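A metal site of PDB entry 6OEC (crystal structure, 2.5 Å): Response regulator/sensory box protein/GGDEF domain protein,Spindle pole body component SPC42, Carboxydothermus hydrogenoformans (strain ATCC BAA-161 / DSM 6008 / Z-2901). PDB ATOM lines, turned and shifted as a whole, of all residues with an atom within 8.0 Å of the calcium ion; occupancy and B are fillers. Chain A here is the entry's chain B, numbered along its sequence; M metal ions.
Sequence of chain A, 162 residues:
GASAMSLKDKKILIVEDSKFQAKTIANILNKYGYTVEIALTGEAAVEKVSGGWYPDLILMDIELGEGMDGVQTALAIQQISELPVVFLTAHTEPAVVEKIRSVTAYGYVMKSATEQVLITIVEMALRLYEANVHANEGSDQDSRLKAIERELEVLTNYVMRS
O of Glu 63 binds the calcium ion (2.3 Å). OD1 of Asp 17 binds the calcium ion, at 2.6 Å. The calcium ion is bound by OD2 of Asp 61, 2.8 Å away. The calcium ion has three donor atoms within binding distance.
Glu 16 touches the calcium ion. Within 4 Å of the calcium ion: Glu 16, Asp 17, Asp 61 and Glu 63.
OD1 of Asp 61 is in salt-bridge range of NZ of Lys 111, at 3.9 Å. OD2 of Asp 61 sits close to OE1 of Glu 16 (2.5 Å). The side-chain carboxylate of Glu 16 sits at hydrogen-bond distance from the backbone NH of Ser 18 (2.8 Å). N of Asp 61 sits at hydrogen-bond distance from O of Val 15.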
ATOM      1  N   VAL A  15       8.920   0.865  11.392  1.00  0.00           N
ATOM      2  CA  VAL A  15       9.462  -0.132  10.494  1.00  0.00           C
ATOM      3  C   VAL A  15      10.517   0.575   9.689  1.00  0.00           C
ATOM      4  O   VAL A  15      10.183   1.383   8.805  1.00  0.00           O
ATOM      5  CB  VAL A  15       8.392  -0.773   9.613  1.00  0.00           C
ATOM      6  CG1 VAL A  15       9.000  -1.886   8.773  1.00  0.00           C
ATOM      7  CG2 VAL A  15       7.254  -1.292  10.474  1.00  0.00           C
ATOM      8  N   GLU A  16      11.786   0.244   9.963  1.00  0.00           N
ATOM      9  CA  GLU A  16      12.931   1.074   9.612  1.00  0.00           C
ATOM     10  C   GLU A  16      14.222   0.264   9.707  1.00  0.00           C
ATOM     11  O   GLU A  16      14.564  -0.196  10.791  1.00  0.00           O
ATOM     12  CB  GLU A  16      12.983   2.255  10.570  1.00  0.00           C
ATOM     13  CG  GLU A  16      14.240   3.066  10.479  1.00  0.00           C
ATOM     14  CD  GLU A  16      14.522   3.465   9.058  1.00  0.00           C
ATOM     15  OE1 GLU A  16      13.601   3.998   8.407  1.00  0.00           O
ATOM     16  OE2 GLU A  16      15.651   3.217   8.601  1.00  0.00           O
ATOM     17  N   ASP A  17      14.961   0.095   8.613  1.00  0.00           N
ATOM     18  CA  ASP A  17      16.102  -0.805   8.763  1.00  0.00           C
ATOM     19  C   ASP A  17      17.294  -0.132   9.417  1.00  0.00           C
ATOM     20  O   ASP A  17      18.045  -0.809  10.139  1.00  0.00           O
ATOM     21  CB  ASP A  17      16.541  -1.388   7.420  1.00  0.00           C
ATOM     22  CG  ASP A  17      16.835  -0.335   6.406  1.00  0.00           C
ATOM     23  OD1 ASP A  17      15.994   0.579   6.287  1.00  0.00           O
ATOM     24  OD2 ASP A  17      17.884  -0.401   5.732  1.00  0.00           O
ATOM     25  N   SER A  18      17.506   1.157   9.218  1.00  0.00           N
ATOM     26  CA  SER A  18      18.604   1.815   9.924  1.00  0.00           C
ATOM     27  C   SER A  18      18.314   1.824  11.423  1.00  0.00           C
ATOM     28  O   SER A  18      17.348   2.448  11.879  1.00  0.00           O
ATOM     29  CB  SER A  18      18.793   3.235   9.436  1.00  0.00           C
ATOM     30  OG  SER A  18      19.516   3.943  10.432  1.00  0.00           O
ATOM     31  N   GLN A  21      18.345   5.529  12.713  1.00  0.00           N
ATOM     32  CA  GLN A  21      17.131   6.286  12.425  1.00  0.00           C
ATOM     33  C   GLN A  21      15.948   5.772  13.253  1.00  0.00           C
ATOM     34  O   GLN A  21      15.145   6.580  13.759  1.00  0.00           O
ATOM     35  CB  GLN A  21      16.851   6.221  10.915  1.00  0.00           C
ATOM     36  CG  GLN A  21      17.792   7.082  10.099  1.00  0.00           C
ATOM     37  CD  GLN A  21      17.658   6.894   8.612  1.00  0.00           C
ATOM     38  OE1 GLN A  21      16.601   6.554   8.092  1.00  0.00           O
ATOM     39  NE2 GLN A  21      18.741   7.132   7.895  1.00  0.00           N
ATOM     40  N   LEU A  40      13.117  -3.922  12.359  1.00  0.00           N
ATOM     41  CA  LEU A  40      14.167  -3.602  11.406  1.00  0.00           C
ATOM     42  C   LEU A  40      13.869  -4.031   9.966  1.00  0.00           C
ATOM     43  O   LEU A  40      14.622  -3.642   9.074  1.00  0.00           O
ATOM     44  CB  LEU A  40      15.487  -4.205  11.861  1.00  0.00           C
ATOM     45  CG  LEU A  40      15.831  -3.683  13.243  1.00  0.00           C
ATOM     46  CD1 LEU A  40      17.018  -4.426  13.815  1.00  0.00           C
ATOM     47  CD2 LEU A  40      16.132  -2.196  13.135  1.00  0.00           C
ATOM     48  N   MET A  60       6.363   3.802   8.505  1.00  0.00           N
ATOM     49  CA  MET A  60       6.992   2.866   7.596  1.00  0.00           C
ATOM     50  C   MET A  60       7.976   3.570   6.663  1.00  0.00           C
ATOM     51  O   MET A  60       7.552   4.295   5.765  1.00  0.00           O
ATOM     52  CB  MET A  60       5.945   2.168   6.735  1.00  0.00           C
ATOM     53  CG  MET A  60       6.543   1.193   5.730  1.00  0.00           C
ATOM     54  SD  MET A  60       6.422  -0.459   6.443  1.00  0.00           S
ATOM     55  CE  MET A  60       4.634  -0.649   6.335  1.00  0.00           C
ATOM     56  N   ASP A  61       9.257   3.264   6.795  1.00  0.00           N
ATOM     57  CA  ASP A  61      10.182   3.746   5.784  1.00  0.00           C
ATOM     58  C   ASP A  61       9.862   3.090   4.431  1.00  0.00           C
ATOM     59  O   ASP A  61       9.654   1.871   4.378  1.00  0.00           O
ATOM     60  CB  ASP A  61      11.614   3.466   6.214  1.00  0.00           C
ATOM     61  CG  ASP A  61      12.627   4.247   5.420  1.00  0.00           C
ATOM     62  OD1 ASP A  61      12.316   4.631   4.260  1.00  0.00           O
ATOM     63  OD2 ASP A  61      13.736   4.482   5.936  1.00  0.00           O
ATOM     64  N   ILE A  62       9.817   3.877   3.338  1.00  0.00           N
ATOM     65  CA  ILE A  62       9.548   3.265   2.031  1.00  0.00           C
ATOM     66  C   ILE A  62      10.700   2.398   1.524  1.00  0.00           C
ATOM     67  O   ILE A  62      10.511   1.619   0.590  1.00  0.00           O
ATOM     68  CB  ILE A  62       9.253   4.216   0.847  1.00  0.00           C
ATOM     69  CG1 ILE A  62       9.869   5.590   1.000  1.00  0.00           C
ATOM     70  CG2 ILE A  62       7.800   4.212   0.493  1.00  0.00           C
ATOM     71  CD1 ILE A  62      11.355   5.590   0.547  1.00  0.00           C
ATOM     72  N   GLU A  63      11.887   2.537   2.088  1.00  0.00           N
ATOM     73  CA  GLU A  63      13.048   1.763   1.643  1.00  0.00           C
ATOM     74  C   GLU A  63      13.607   1.050   2.847  1.00  0.00           C
ATOM     75  O   GLU A  63      13.941   1.690   3.850  1.00  0.00           O
ATOM     76  CB  GLU A  63      14.096   2.667   0.987  1.00  0.00           C
ATOM     77  CG  GLU A  63      13.886   2.860  -0.503  1.00  0.00           C
ATOM     78  CD  GLU A  63      14.538   4.127  -1.049  1.00  0.00           C
ATOM     79  OE1 GLU A  63      13.970   4.756  -1.984  1.00  0.00           O
ATOM     80  OE2 GLU A  63      15.626   4.497  -0.518  1.00  0.00           O
ATOM     81  N   LEU A  64      13.680  -0.282   2.769  1.00  0.00           N
ATOM     82  CA  LEU A  64      13.892  -1.115   3.951  1.00  0.00           C
ATOM     83  C   LEU A  64      15.032  -2.114   3.745  1.00  0.00           C
ATOM     84  O   LEU A  64      15.067  -3.172   4.384  1.00  0.00           O
ATOM     85  CB  LEU A  64      12.611  -1.849   4.343  1.00  0.00           C
ATOM     86  CG  LEU A  64      11.575  -0.962   4.994  1.00  0.00           C
ATOM     87  CD1 LEU A  64      10.280  -1.719   5.201  1.00  0.00           C
ATOM     88  CD2 LEU A  64      12.173  -0.481   6.306  1.00  0.00           C
ATOM     89  N   GLY A  65      15.971  -1.789   2.867  1.00  0.00           N
ATOM     90  CA  GLY A  65      17.066  -2.701   2.676  1.00  0.00           C
ATOM     91  C   GLY A  65      16.730  -3.882   1.786  1.00  0.00           C
ATOM     92  O   GLY A  65      15.967  -3.747   0.816  1.00  0.00           O
ATOM     93  N   LEU A  88       7.542   7.099   6.093  1.00  0.00           N
ATOM     94  CA  LEU A  88       8.721   7.930   6.180  1.00  0.00           C
ATOM     95  C   LEU A  88       9.400   8.002   4.815  1.00  0.00           C
ATOM     96  O   LEU A  88       9.665   6.963   4.205  1.00  0.00           O
ATOM     97  CB  LEU A  88       9.709   7.352   7.193  1.00  0.00           C
ATOM     98  CG  LEU A  88       9.282   7.548   8.621  1.00  0.00           C
ATOM     99  CD1 LEU A  88      10.075   6.660   9.475  1.00  0.00           C
ATOM    100  CD2 LEU A  88       9.608   8.960   8.950  1.00  0.00           C
ATOM    101  N   LYS A 111      11.651  12.524   6.324  1.00  0.00           N
ATOM    102  CA  LYS A 111      12.698  12.143   7.268  1.00  0.00           C
ATOM    103  C   LYS A 111      13.274  13.374   7.966  1.00  0.00           C
ATOM    104  O   LYS A 111      13.687  13.285   9.135  1.00  0.00           O
ATOM    105  CB  LYS A 111      13.796  11.364   6.565  1.00  0.00           C
ATOM    106  CG  LYS A 111      13.679   9.861   6.721  1.00  0.00           C
ATOM    107  CD  LYS A 111      14.021   9.137   5.426  1.00  0.00           C
ATOM    108  CE  LYS A 111      13.918   7.628   5.563  1.00  0.00           C
ATOM    109  NZ  LYS A 111      15.220   6.934   5.404  1.00  0.00           N
HETATM  110 CA    CA M   1      15.662   2.752   4.917  1.00  0.00          CA
